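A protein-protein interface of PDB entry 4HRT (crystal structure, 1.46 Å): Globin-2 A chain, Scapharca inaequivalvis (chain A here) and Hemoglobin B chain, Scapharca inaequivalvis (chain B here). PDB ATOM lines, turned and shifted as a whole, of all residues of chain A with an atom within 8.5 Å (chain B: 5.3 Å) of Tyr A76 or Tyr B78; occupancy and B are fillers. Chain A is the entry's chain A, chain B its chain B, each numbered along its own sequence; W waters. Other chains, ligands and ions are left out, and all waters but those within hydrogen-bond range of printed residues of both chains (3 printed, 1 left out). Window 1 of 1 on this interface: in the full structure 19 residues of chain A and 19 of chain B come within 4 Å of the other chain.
Of the printed residues of chain B, Tyr A76 touches Tyr B78, Gln B81, Asn B82, Asp B85 and Arg B92. Of the printed residues of chain A, Tyr B78 touches Tyr A76, Asn A79, Asn A80, Asp A83 and Arg A90. No residue of chain A comes within 4 Å of Ala B79. Printed residues of chain B within 4 Å of Asn A80: Ile B74, Thr B75 and Tyr B78. Of the printed residues of chain A, Arg B92 touches Ile A30, Ile A72 and Tyr A76. Printed residues of chain B within 4 Å of Ile A30: Arg B92 (3.5 Å). Of the printed residues of chain B, Ile A72 touches Asn B82 and Arg B92. Of the printed residues of chain B, Thr A73 touches Asn B82. The nearest residue of chain A that does not touch Tyr B78 is Ala A77 (5.7 Å). The nearest printed residue of chain A that does not touch Asp B85 is Ile A30 (5.7 Å).
Water W1 lies within hydrogen-bond range of the side-chain hydroxyl of Thr B75 (2.8 Å) and the backbone carbonyl oxygen of Val A94 (2.9 Å). Water W3 bridges NH1 of Arg A90 (2.9 Å) and OH of Tyr B78 (3.3 Å). Water W2 bridges the backbone NH of Met B32 (3.3 Å) and the guanidinium group of Arg A90 (3.4 Å).
Of the 23 printed residues of chain A, 8 touch a printed residue of chain B. Of the 12 printed residues of chain B, 7 touch a printed residue of chain A. Printed residues of chain B that touch a printed residue of chain A: Ile B74, Thr B75, Tyr B78, Gln B81, Asn B82, Asp B85 and Arg B92. Hydrophobic or aromatic side chains of chain B that line the printed part of chain A: Ile B74 and Tyr B78. Among the printed residues, no Asp or Glu carboxylate lies within 4 Å of a Lys or Arg side-chain nitrogen of the other chain.
The backbone carbonyl oxygen of Gly A69 sits at hydrogen-bond distance from the side-chain hydroxyl of Thr A73 (2.8 Å). The backbone carbonyl oxygen (O) of Ile A72 sits at hydrogen-bond distance from the side-chain hydroxyl (OG1) of Thr A75 (2.8 Å). O of Asn A80 is in hydrogen-bond range of OG of Ser A84. The side-chain amide oxygen of Asn A80 sits at hydrogen-bond distance from the guanidinium group of Arg A90 (3.0 Å). The side-chain hydroxyl (OG) of Ser A84 lies within hydrogen-bond range of the guanidinium group (NE) of Arg A90 (2.8 Å). NE2 of Gln B81 is in hydrogen-bond range of OD1 of Asp B85, 3.0 Å away.
Arg B92 touches Ile A30. OD1 of Asn B82 touches CG2 of Ile A72, at 3.7 Å. CG of Arg B92 touches CD1 of Ile A72, 3.9 Å away. O of Tyr B78 touches CD1 of Tyr A76 (3.7 Å). Tyr A76 touches Gln B81. Tyr A76 touches Asn B82 (CE2 to CG, 3.5 Å). Asn A79 touches Tyr B78. Asn A80 touches Ile B74 (OD1 to CG2, 3.5 Å). Tyr B78 touches Asn A80. Arg A90 touches Ile B74 (NH2 to CG2, 3.6 Å).
The side-chain hydroxyl (OG1) of Thr A73 lies within hydrogen-bond range of the side-chain amide nitrogen (ND2) of Asn B82 (3.2 Å). The side-chain hydroxyl of Tyr A76 is in hydrogen-bond range of the side-chain carboxylate of Asp B85 (2.7 Å). The side-chain hydroxyl of Tyr A76 lies within hydrogen-bond range of the guanidinium group of Arg B92 (3.4 Å). The side-chain hydroxyl (OG1) of Thr B75 is in hydrogen-bond range of the side-chain amide nitrogen (ND2) of Asn A80 (3.4 Å). OD2 of Asp A83 is in hydrogen-bond range of OH of Tyr B78 (2.6 Å). The guanidinium group (NH2) of Arg A90 is in hydrogen-bond range of the side-chain hydroxyl (OH) of Tyr B78 (3.0 Å).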
ATOM      1  N   TRP A  23     -30.319 -21.594 -21.361  1.00  0.00           N
ATOM      2  CA  TRP A  23     -29.920 -20.187 -21.449  1.00  0.00           C
ATOM      3  C   TRP A  23     -29.629 -19.778 -22.900  1.00  0.00           C
ATOM      4  O   TRP A  23     -30.023 -18.706 -23.346  1.00  0.00           O
ATOM      5  CB  TRP A  23     -28.729 -19.858 -20.531  1.00  0.00           C
ATOM      6  CG  TRP A  23     -28.249 -18.448 -20.757  1.00  0.00           C
ATOM      7  CD1 TRP A  23     -27.105 -18.055 -21.405  1.00  0.00           C
ATOM      8  CD2 TRP A  23     -28.947 -17.247 -20.414  1.00  0.00           C
ATOM      9  NE1 TRP A  23     -27.031 -16.681 -21.446  1.00  0.00           N
ATOM     10  CE2 TRP A  23     -28.148 -16.161 -20.843  1.00  0.00           C
ATOM     11  CE3 TRP A  23     -30.160 -16.982 -19.758  1.00  0.00           C
ATOM     12  CZ2 TRP A  23     -28.537 -14.825 -20.664  1.00  0.00           C
ATOM     13  CZ3 TRP A  23     -30.536 -15.641 -19.565  1.00  0.00           C
ATOM     14  CH2 TRP A  23     -29.723 -14.590 -20.014  1.00  0.00           C
ATOM     15  N   ILE A  30     -33.735 -11.890 -24.977  1.00  0.00           N
ATOM     16  CA  ILE A  30     -33.711 -11.711 -23.520  1.00  0.00           C
ATOM     17  C   ILE A  30     -34.869 -10.839 -23.034  1.00  0.00           C
ATOM     18  O   ILE A  30     -35.427 -11.116 -21.978  1.00  0.00           O
ATOM     19  CB  ILE A  30     -32.338 -11.261 -22.946  1.00  0.00           C
ATOM     20  CG1 ILE A  30     -31.909  -9.888 -23.466  1.00  0.00           C
ATOM     21  CG2 ILE A  30     -31.262 -12.319 -23.160  1.00  0.00           C
ATOM     22  CD1 ILE A  30     -32.235  -8.770 -22.490  1.00  0.00           C
ATOM     23  N   GLU A  31     -35.263  -9.836 -23.821  1.00  0.00           N
ATOM     24  CA  GLU A  31     -36.381  -8.975 -23.419  1.00  0.00           C
ATOM     25  C   GLU A  31     -37.691  -9.764 -23.377  1.00  0.00           C
ATOM     26  O   GLU A  31     -38.428  -9.682 -22.389  1.00  0.00           O
ATOM     27  CB  GLU A  31     -36.504  -7.744 -24.316  1.00  0.00           C
ATOM     28  CG  GLU A  31     -37.601  -6.795 -23.874  1.00  0.00           C
ATOM     29  CD  GLU A  31     -37.945  -5.751 -24.920  1.00  0.00           C
ATOM     30  OE1 GLU A  31     -37.131  -5.485 -25.832  1.00  0.00           O
ATOM     31  OE2 GLU A  31     -39.054  -5.206 -24.834  1.00  0.00           O
ATOM     32  N   GLY A  34     -37.603 -12.173 -20.343  1.00  0.00           N
ATOM     33  CA  GLY A  34     -37.836 -11.488 -19.064  1.00  0.00           C
ATOM     34  C   GLY A  34     -39.305 -11.165 -18.863  1.00  0.00           C
ATOM     35  O   GLY A  34     -39.856 -11.405 -17.790  1.00  0.00           O
ATOM     36  N   GLY A  69     -38.309  -2.378 -17.802  1.00  0.00           N
ATOM     37  CA  GLY A  69     -36.928  -2.217 -17.326  1.00  0.00           C
ATOM     38  C   GLY A  69     -36.523  -3.288 -16.320  1.00  0.00           C
ATOM     39  O   GLY A  69     -35.388  -3.803 -16.356  1.00  0.00           O
ATOM     40  N   HIS A  70     -37.446  -3.637 -15.420  1.00  0.00           N
ATOM     41  CA  HIS A  70     -37.176  -4.708 -14.470  1.00  0.00           C
ATOM     42  C   HIS A  70     -36.992  -6.064 -15.168  1.00  0.00           C
ATOM     43  O   HIS A  70     -36.028  -6.783 -14.879  1.00  0.00           O
ATOM     44  CB  HIS A  70     -38.255  -4.813 -13.386  1.00  0.00           C
ATOM     45  CG  HIS A  70     -38.075  -6.010 -12.509  1.00  0.00           C
ATOM     46  ND1 HIS A  70     -37.086  -6.087 -11.549  1.00  0.00           N
ATOM     47  CD2 HIS A  70     -38.704  -7.210 -12.502  1.00  0.00           C
ATOM     48  CE1 HIS A  70     -37.145  -7.268 -10.960  1.00  0.00           C
ATOM     49  NE2 HIS A  70     -38.111  -7.971 -11.527  1.00  0.00           N
ATOM     50  N   ALA A  71     -37.908  -6.399 -16.082  1.00  0.00           N
ATOM     51  CA  ALA A  71     -37.884  -7.683 -16.798  1.00  0.00           C
ATOM     52  C   ALA A  71     -36.584  -7.866 -17.577  1.00  0.00           C
ATOM     53  O   ALA A  71     -35.971  -8.956 -17.536  1.00  0.00           O
ATOM     54  CB  ALA A  71     -39.080  -7.775 -17.736  1.00  0.00           C
ATOM     55  N   ILE A  72     -36.153  -6.815 -18.276  1.00  0.00           N
ATOM     56  CA  ILE A  72     -34.872  -6.867 -19.004  1.00  0.00           C
ATOM     57  C   ILE A  72     -33.704  -7.038 -18.022  1.00  0.00           C
ATOM     58  O   ILE A  72     -32.827  -7.899 -18.203  1.00  0.00           O
ATOM     59  CB  ILE A  72     -34.640  -5.603 -19.865  1.00  0.00           C
ATOM     60  CG1 ILE A  72     -35.663  -5.533 -21.013  1.00  0.00           C
ATOM     61  CG2 ILE A  72     -33.197  -5.547 -20.385  1.00  0.00           C
ATOM     62  CD1 ILE A  72     -35.709  -4.198 -21.728  1.00  0.00           C
ATOM     63  N   THR A  73     -33.679  -6.224 -16.977  1.00  0.00           N
ATOM     64  CA  THR A  73     -32.574  -6.233 -16.018  1.00  0.00           C
ATOM     65  C   THR A  73     -32.428  -7.571 -15.283  1.00  0.00           C
ATOM     66  O   THR A  73     -31.306  -8.039 -15.055  1.00  0.00           O
ATOM     67  CB  THR A  73     -32.719  -5.017 -15.074  1.00  0.00           C
ATOM     68  OG1 THR A  73     -32.654  -3.840 -15.883  1.00  0.00           O
ATOM     69  CG2 THR A  73     -31.606  -4.947 -14.024  1.00  0.00           C
ATOM     70  N   LEU A  74     -33.553  -8.202 -14.951  1.00  0.00           N
ATOM     71  CA  LEU A  74     -33.548  -9.512 -14.302  1.00  0.00           C
ATOM     72  C   LEU A  74     -32.704 -10.527 -15.094  1.00  0.00           C
ATOM     73  O   LEU A  74     -31.972 -11.324 -14.502  1.00  0.00           O
ATOM     74  CB  LEU A  74     -34.991 -10.014 -14.105  1.00  0.00           C
ATOM     75  CG  LEU A  74     -35.255 -11.447 -13.627  1.00  0.00           C
ATOM     76  CD1 LEU A  74     -36.576 -11.537 -12.880  1.00  0.00           C
ATOM     77  CD2 LEU A  74     -35.207 -12.435 -14.793  1.00  0.00           C
ATOM     78  N   THR A  75     -32.801 -10.475 -16.420  1.00  0.00           N
ATOM     79  CA  THR A  75     -32.110 -11.480 -17.249  1.00  0.00           C
ATOM     80  C   THR A  75     -30.590 -11.358 -17.177  1.00  0.00           C
ATOM     81  O   THR A  75     -29.890 -12.363 -17.386  1.00  0.00           O
ATOM     82  CB  THR A  75     -32.568 -11.479 -18.727  1.00  0.00           C
ATOM     83  OG1 THR A  75     -32.085 -10.306 -19.394  1.00  0.00           O
ATOM     84  CG2 THR A  75     -34.093 -11.598 -18.849  1.00  0.00           C
ATOM     85  N   TYR A  76     -30.072 -10.161 -16.871  1.00  0.00           N
ATOM     86  CA  TYR A  76     -28.613  -9.981 -16.751  1.00  0.00           C
ATOM     87  C   TYR A  76     -28.036 -10.609 -15.481  1.00  0.00           C
ATOM     88  O   TYR A  76     -26.844 -10.949 -15.450  1.00  0.00           O
ATOM     89  CB  TYR A  76     -28.178  -8.512 -16.934  1.00  0.00           C
ATOM     90  CG  TYR A  76     -28.382  -8.061 -18.359  1.00  0.00           C
ATOM     91  CD1 TYR A  76     -27.382  -8.254 -19.329  1.00  0.00           C
ATOM     92  CD2 TYR A  76     -29.597  -7.514 -18.771  1.00  0.00           C
ATOM     93  CE1 TYR A  76     -27.578  -7.874 -20.646  1.00  0.00           C
ATOM     94  CE2 TYR A  76     -29.800  -7.141 -20.087  1.00  0.00           C
ATOM     95  CZ  TYR A  76     -28.792  -7.328 -21.022  1.00  0.00           C
ATOM     96  OH  TYR A  76     -29.019  -6.955 -22.324  1.00  0.00           O
ATOM     97  N   ALA A  77     -28.868 -10.787 -14.452  1.00  0.00           N
ATOM     98  CA  ALA A  77     -28.467 -11.596 -13.304  1.00  0.00           C
ATOM     99  C   ALA A  77     -28.383 -13.077 -13.716  1.00  0.00           C
ATOM    100  O   ALA A  77     -27.407 -13.762 -13.372  1.00  0.00           O
ATOM    101  CB  ALA A  77     -29.425 -11.402 -12.127  1.00  0.00           C
ATOM    102  N   LEU A  78     -29.392 -13.564 -14.448  1.00  0.00           N
ATOM    103  CA  LEU A  78     -29.360 -14.941 -14.971  1.00  0.00           C
ATOM    104  C   LEU A  78     -28.127 -15.158 -15.845  1.00  0.00           C
ATOM    105  O   LEU A  78     -27.481 -16.198 -15.737  1.00  0.00           O
ATOM    106  CB  LEU A  78     -30.645 -15.286 -15.737  1.00  0.00           C
ATOM    107  CG  LEU A  78     -31.943 -15.264 -14.912  1.00  0.00           C
ATOM    108  CD1 LEU A  78     -33.119 -15.661 -15.795  1.00  0.00           C
ATOM    109  CD2 LEU A  78     -31.856 -16.161 -13.678  1.00  0.00           C
ATOM    110  N   ASN A  79     -27.806 -14.179 -16.696  1.00  0.00           N
ATOM    111  CA  ASN A  79     -26.623 -14.254 -17.564  1.00  0.00           C
ATOM    112  C   ASN A  79     -25.354 -14.419 -16.740  1.00  0.00           C
ATOM    113  O   ASN A  79     -24.519 -15.283 -17.035  1.00  0.00           O
ATOM    114  CB  ASN A  79     -26.545 -12.981 -18.418  1.00  0.00           C
ATOM    115  CG  ASN A  79     -25.536 -13.061 -19.557  1.00  0.00           C
ATOM    116  OD1 ASN A  79     -24.783 -14.039 -19.726  1.00  0.00           O
ATOM    117  ND2 ASN A  79     -25.509 -12.001 -20.345  1.00  0.00           N
ATOM    118  N   ASN A  80     -25.212 -13.600 -15.703  1.00  0.00           N
ATOM    119  CA  ASN A  80     -24.084 -13.670 -14.781  1.00  0.00           C
ATOM    120  C   ASN A  80     -24.027 -15.038 -14.087  1.00  0.00           C
ATOM    121  O   ASN A  80     -22.952 -15.673 -14.043  1.00  0.00           O
ATOM    122  CB  ASN A  80     -24.253 -12.515 -13.782  1.00  0.00           C
ATOM    123  CG  ASN A  80     -23.059 -12.291 -12.875  1.00  0.00           C
ATOM    124  OD1 ASN A  80     -22.085 -13.044 -12.858  1.00  0.00           O
ATOM    125  ND2 ASN A  80     -23.159 -11.226 -12.062  1.00  0.00           N
ATOM    126  N   PHE A  81     -25.165 -15.526 -13.581  1.00  0.00           N
ATOM    127  CA  PHE A  81     -25.192 -16.861 -12.940  1.00  0.00           C
ATOM    128  C   PHE A  81     -24.687 -17.953 -13.905  1.00  0.00           C
ATOM    129  O   PHE A  81     -23.852 -18.779 -13.527  1.00  0.00           O
ATOM    130  CB  PHE A  81     -26.600 -17.262 -12.463  1.00  0.00           C
ATOM    131  CG  PHE A  81     -27.198 -16.395 -11.372  1.00  0.00           C
ATOM    132  CD1 PHE A  81     -26.448 -15.470 -10.632  1.00  0.00           C
ATOM    133  CD2 PHE A  81     -28.540 -16.562 -11.075  1.00  0.00           C
ATOM    134  CE1 PHE A  81     -27.058 -14.697  -9.632  1.00  0.00           C
ATOM    135  CE2 PHE A  81     -29.149 -15.800 -10.077  1.00  0.00           C
ATOM    136  CZ  PHE A  81     -28.406 -14.878  -9.358  1.00  0.00           C
ATOM    137  N   VAL A  82     -25.188 -17.950 -15.143  1.00  0.00           N
ATOM    138  CA  VAL A  82     -24.784 -18.975 -16.124  1.00  0.00           C
ATOM    139  C   VAL A  82     -23.291 -18.859 -16.421  1.00  0.00           C
ATOM    140  O   VAL A  82     -22.606 -19.887 -16.537  1.00  0.00           O
ATOM    141  CB  VAL A  82     -25.644 -18.853 -17.406  1.00  0.00           C
ATOM    142  CG1 VAL A  82     -25.115 -19.740 -18.529  1.00  0.00           C
ATOM    143  CG2 VAL A  82     -27.079 -19.258 -17.120  1.00  0.00           C
ATOM    144  N   ASP A  83     -22.779 -17.635 -16.523  1.00  0.00           N
ATOM    145  CA  ASP A  83     -21.349 -17.397 -16.770  1.00  0.00           C
ATOM    146  C   ASP A  83     -20.464 -17.758 -15.568  1.00  0.00           C
ATOM    147  O   ASP A  83     -19.223 -17.720 -15.666  1.00  0.00           O
ATOM    148  CB  ASP A  83     -21.090 -15.932 -17.168  1.00  0.00           C
ATOM    149  CG  ASP A  83     -21.563 -15.590 -18.569  1.00  0.00           C
ATOM    150  OD1 ASP A  83     -21.892 -16.502 -19.355  1.00  0.00           O
ATOM    151  OD2 ASP A  83     -21.601 -14.375 -18.884  1.00  0.00           O
ATOM    152  N   SER A  84     -21.098 -18.106 -14.445  1.00  0.00           N
ATOM    153  CA  SER A  84     -20.398 -18.453 -13.205  1.00  0.00           C
ATOM    154  C   SER A  84     -20.312 -19.955 -12.949  1.00  0.00           C
ATOM    155  O   SER A  84     -19.670 -20.364 -11.982  1.00  0.00           O
ATOM    156  CB  SER A  84     -21.100 -17.812 -11.993  1.00  0.00           C
ATOM    157  OG  SER A  84     -21.133 -16.400 -12.090  1.00  0.00           O
ATOM    158  N   ARG A  90     -16.908 -18.238  -7.786  1.00  0.00           N
ATOM    159  CA  ARG A  90     -17.620 -17.139  -8.448  1.00  0.00           C
ATOM    160  C   ARG A  90     -19.132 -17.225  -8.261  1.00  0.00           C
ATOM    161  O   ARG A  90     -19.764 -16.216  -7.920  1.00  0.00           O
ATOM    162  CB  ARG A  90     -17.282 -17.044  -9.946  1.00  0.00           C
ATOM    163  CG  ARG A  90     -18.074 -15.920 -10.620  1.00  0.00           C
ATOM    164  CD  ARG A  90     -17.634 -15.622 -12.050  1.00  0.00           C
ATOM    165  NE  ARG A  90     -18.750 -15.004 -12.781  1.00  0.00           N
ATOM    166  CZ  ARG A  90     -18.645 -14.399 -13.961  1.00  0.00           C
ATOM    167  NH1 ARG A  90     -17.454 -14.265 -14.552  1.00  0.00           N
ATOM    168  NH2 ARG A  90     -19.736 -13.926 -14.563  1.00  0.00           N
ATOM    169  N   VAL A  94     -21.134 -14.132  -6.431  1.00  0.00           N
ATOM    170  CA  VAL A  94     -22.144 -13.462  -7.270  1.00  0.00           C
ATOM    171  C   VAL A  94     -23.550 -13.641  -6.686  1.00  0.00           C
ATOM    172  O   VAL A  94     -24.331 -12.678  -6.643  1.00  0.00           O
ATOM    173  CB  VAL A  94     -22.036 -13.948  -8.739  1.00  0.00           C
ATOM    174  CG1 VAL A  94     -23.306 -13.666  -9.534  1.00  0.00           C
ATOM    175  CG2 VAL A  94     -20.813 -13.305  -9.382  1.00  0.00           C
ATOM    176  N   PHE A  98     -25.984 -10.734  -5.141  1.00  0.00           N
ATOM    177  CA  PHE A  98     -27.368 -10.664  -5.625  1.00  0.00           C
ATOM    178  C   PHE A  98     -28.372 -10.703  -4.475  1.00  0.00           C
ATOM    179  O   PHE A  98     -29.396 -10.002  -4.514  1.00  0.00           O
ATOM    180  CB  PHE A  98     -27.585 -11.854  -6.572  1.00  0.00           C
ATOM    181  CG  PHE A  98     -29.012 -12.075  -6.993  1.00  0.00           C
ATOM    182  CD1 PHE A  98     -29.864 -12.896  -6.242  1.00  0.00           C
ATOM    183  CD2 PHE A  98     -29.503 -11.482  -8.150  1.00  0.00           C
ATOM    184  CE1 PHE A  98     -31.180 -13.111  -6.627  1.00  0.00           C
ATOM    185  CE2 PHE A  98     -30.812 -11.709  -8.549  1.00  0.00           C
ATOM    186  CZ  PHE A  98     -31.653 -12.522  -7.793  1.00  0.00           C
ATOM    187  N   MET B  32     -14.610 -10.067 -18.122  1.00  0.00           N
ATOM    188  CA  MET B  32     -15.587  -9.307 -17.321  1.00  0.00           C
ATOM    189  C   MET B  32     -15.072  -9.137 -15.894  1.00  0.00           C
ATOM    190  O   MET B  32     -15.111  -8.022 -15.351  1.00  0.00           O
ATOM    191  CB  MET B  32     -16.959  -9.995 -17.334  1.00  0.00           C
ATOM    192  CG  MET B  32     -17.633 -10.045 -18.697  1.00  0.00           C
ATOM    193  SD  MET B  32     -18.397  -8.486 -19.208  1.00  0.00           S
ATOM    194  CE  MET B  32     -20.008  -8.584 -18.405  1.00  0.00           C
ATOM    195  N   ILE B  74     -17.799  -7.957 -10.689  1.00  0.00           N
ATOM    196  CA  ILE B  74     -18.349  -8.777 -11.783  1.00  0.00           C
ATOM    197  C   ILE B  74     -19.759  -8.276 -12.140  1.00  0.00           C
ATOM    198  O   ILE B  74     -20.082  -8.028 -13.317  1.00  0.00           O
ATOM    199  CB  ILE B  74     -18.415 -10.267 -11.393  1.00  0.00           C
ATOM    200  CG1 ILE B  74     -16.994 -10.838 -11.206  1.00  0.00           C
ATOM    201  CG2 ILE B  74     -19.198 -11.067 -12.436  1.00  0.00           C
ATOM    202  CD1 ILE B  74     -16.952 -12.196 -10.524  1.00  0.00           C
ATOM    203  N   THR B  75     -20.585  -8.078 -11.108  1.00  0.00           N
ATOM    204  CA  THR B  75     -21.985  -7.684 -11.294  1.00  0.00           C
ATOM    205  C   THR B  75     -22.120  -6.315 -11.992  1.00  0.00           C
ATOM    206  O   THR B  75     -22.985  -6.153 -12.861  1.00  0.00           O
ATOM    207  CB  THR B  75     -22.716  -7.748  -9.934  1.00  0.00           C
ATOM    208  OG1 THR B  75     -22.626  -9.098  -9.446  1.00  0.00           O
ATOM    209  CG2 THR B  75     -24.198  -7.330 -10.047  1.00  0.00           C
ATOM    210  N   LEU B  76     -21.250  -5.357 -11.648  1.00  0.00           N
ATOM    211  CA  LEU B  76     -21.230  -4.045 -12.304  1.00  0.00           C
ATOM    212  C   LEU B  76     -21.114  -4.187 -13.826  1.00  0.00           C
ATOM    213  O   LEU B  76     -21.754  -3.459 -14.592  1.00  0.00           O
ATOM    214  CB  LEU B  76     -20.080  -3.189 -11.749  1.00  0.00           C
ATOM    215  CG  LEU B  76     -19.822  -1.804 -12.354  1.00  0.00           C
ATOM    216  CD1 LEU B  76     -19.276  -0.849 -11.312  1.00  0.00           C
ATOM    217  CD2 LEU B  76     -18.889  -1.850 -13.558  1.00  0.00           C
ATOM    218  N   MET B  77     -20.277  -5.133 -14.269  1.00  0.00           N
ATOM    219  CA  MET B  77     -20.041  -5.281 -15.705  1.00  0.00           C
ATOM    220  C   MET B  77     -21.277  -5.737 -16.474  1.00  0.00           C
ATOM    221  O   MET B  77     -21.422  -5.406 -17.655  1.00  0.00           O
ATOM    222  CB  MET B  77     -18.857  -6.224 -15.942  1.00  0.00           C
ATOM    223  CG  MET B  77     -17.532  -5.638 -15.449  1.00  0.00           C
ATOM    224  SD  MET B  77     -16.912  -4.255 -16.449  1.00  0.00           S
ATOM    225  CE  MET B  77     -16.328  -5.145 -17.886  1.00  0.00           C
ATOM    226  N   TYR B  78     -22.167  -6.477 -15.813  1.00  0.00           N
ATOM    227  CA  TYR B  78     -23.437  -6.872 -16.438  1.00  0.00           C
ATOM    228  C   TYR B  78     -24.461  -5.722 -16.547  1.00  0.00           C
ATOM    229  O   TYR B  78     -25.383  -5.789 -17.363  1.00  0.00           O
ATOM    230  CB  TYR B  78     -24.036  -8.138 -15.794  1.00  0.00           C
ATOM    231  CG  TYR B  78     -23.203  -9.374 -16.106  1.00  0.00           C
ATOM    232  CD1 TYR B  78     -22.084  -9.690 -15.334  1.00  0.00           C
ATOM    233  CD2 TYR B  78     -23.512 -10.191 -17.199  1.00  0.00           C
ATOM    234  CE1 TYR B  78     -21.290 -10.788 -15.638  1.00  0.00           C
ATOM    235  CE2 TYR B  78     -22.735 -11.305 -17.500  1.00  0.00           C
ATOM    236  CZ  TYR B  78     -21.629 -11.598 -16.711  1.00  0.00           C
ATOM    237  OH  TYR B  78     -20.845 -12.683 -17.001  1.00  0.00           O
ATOM    238  N   ALA B  79     -24.293  -4.662 -15.759  1.00  0.00           N
ATOM    239  CA  ALA B  79     -25.110  -3.460 -15.979  1.00  0.00           C
ATOM    240  C   ALA B  79     -24.595  -2.705 -17.199  1.00  0.00           C
ATOM    241  O   ALA B  79     -25.378  -2.216 -18.028  1.00  0.00           O
ATOM    242  CB  ALA B  79     -25.105  -2.566 -14.748  1.00  0.00           C
ATOM    243  N   LEU B  80     -23.273  -2.637 -17.351  1.00  0.00           N
ATOM    244  CA  LEU B  80     -22.708  -2.061 -18.570  1.00  0.00           C
ATOM    245  C   LEU B  80     -23.139  -2.831 -19.827  1.00  0.00           C
ATOM    246  O   LEU B  80     -23.502  -2.214 -20.835  1.00  0.00           O
ATOM    247  CB  LEU B  80     -21.185  -1.917 -18.488  1.00  0.00           C
ATOM    248  CG  LEU B  80     -20.677  -0.903 -17.438  1.00  0.00           C
ATOM    249  CD1 LEU B  80     -19.154  -0.903 -17.414  1.00  0.00           C
ATOM    250  CD2 LEU B  80     -21.224   0.518 -17.630  1.00  0.00           C
ATOM    251  N   GLN B  81     -23.142  -4.167 -19.760  1.00  0.00           N
ATOM    252  CA  GLN B  81     -23.629  -4.974 -20.890  1.00  0.00           C
ATOM    253  C   GLN B  81     -25.082  -4.621 -21.253  1.00  0.00           C
ATOM    254  O   GLN B  81     -25.422  -4.456 -22.425  1.00  0.00           O
ATOM    255  CB  GLN B  81     -23.530  -6.467 -20.577  1.00  0.00           C
ATOM    256  CG  GLN B  81     -23.928  -7.379 -21.747  1.00  0.00           C
ATOM    257  CD  GLN B  81     -22.909  -7.363 -22.880  1.00  0.00           C
ATOM    258  OE1 GLN B  81     -21.742  -7.650 -22.667  1.00  0.00           O
ATOM    259  NE2 GLN B  81     -23.354  -7.025 -24.091  1.00  0.00           N
ATOM    260  N   ASN B  82     -25.926  -4.507 -20.228  1.00  0.00           N
ATOM    261  CA  ASN B  82     -27.324  -4.113 -20.376  1.00  0.00           C
ATOM    262  C   ASN B  82     -27.426  -2.748 -21.102  1.00  0.00           C
ATOM    263  O   ASN B  82     -28.145  -2.633 -22.114  1.00  0.00           O
ATOM    264  CB  ASN B  82     -27.906  -4.095 -18.946  1.00  0.00           C
ATOM    265  CG  ASN B  82     -29.418  -3.889 -18.861  1.00  0.00           C
ATOM    266  OD1 ASN B  82     -30.100  -3.520 -19.820  1.00  0.00           O
ATOM    267  ND2 ASN B  82     -29.946  -4.099 -17.646  1.00  0.00           N
ATOM    268  N   ASP B  85     -26.377  -3.135 -24.776  1.00  0.00           N
ATOM    269  CA  ASP B  85     -27.427  -3.851 -25.525  1.00  0.00           C
ATOM    270  C   ASP B  85     -28.674  -3.010 -25.830  1.00  0.00           C
ATOM    271  O   ASP B  85     -29.519  -3.418 -26.627  1.00  0.00           O
ATOM    272  CB  ASP B  85     -27.855  -5.123 -24.775  1.00  0.00           C
ATOM    273  CG  ASP B  85     -26.784  -6.207 -24.768  1.00  0.00           C
ATOM    274  OD1 ASP B  85     -25.816  -6.122 -25.557  1.00  0.00           O
ATOM    275  OD2 ASP B  85     -26.927  -7.142 -23.947  1.00  0.00           O
ATOM    276  N   ARG B  92     -36.036   1.403 -24.823  1.00  0.00           N
ATOM    277  CA  ARG B  92     -35.301   0.414 -24.054  1.00  0.00           C
ATOM    278  C   ARG B  92     -34.190   1.058 -23.210  1.00  0.00           C
ATOM    279  O   ARG B  92     -34.085   0.781 -22.006  1.00  0.00           O
ATOM    280  CB  ARG B  92     -34.735  -0.677 -24.973  1.00  0.00           C
ATOM    281  CG  ARG B  92     -33.977  -1.756 -24.219  1.00  0.00           C
ATOM    282  CD  ARG B  92     -33.587  -2.901 -25.142  1.00  0.00           C
ATOM    283  NE  ARG B  92     -32.667  -3.830 -24.491  1.00  0.00           N
ATOM    284  CZ  ARG B  92     -32.422  -5.067 -24.922  1.00  0.00           C
ATOM    285  NH1 ARG B  92     -33.043  -5.546 -25.994  1.00  0.00           N
ATOM    286  NH2 ARG B  92     -31.550  -5.827 -24.274  1.00  0.00           N
HETATM  287  O   HOH W   1     -24.873 -10.536  -8.506  1.00  0.00           O
HETATM  288  O   HOH W   2     -14.903 -12.936 -16.447  1.00  0.00           O
HETATM  289  O   HOH W   3     -17.774 -13.768 -17.435  1.00  0.00           O
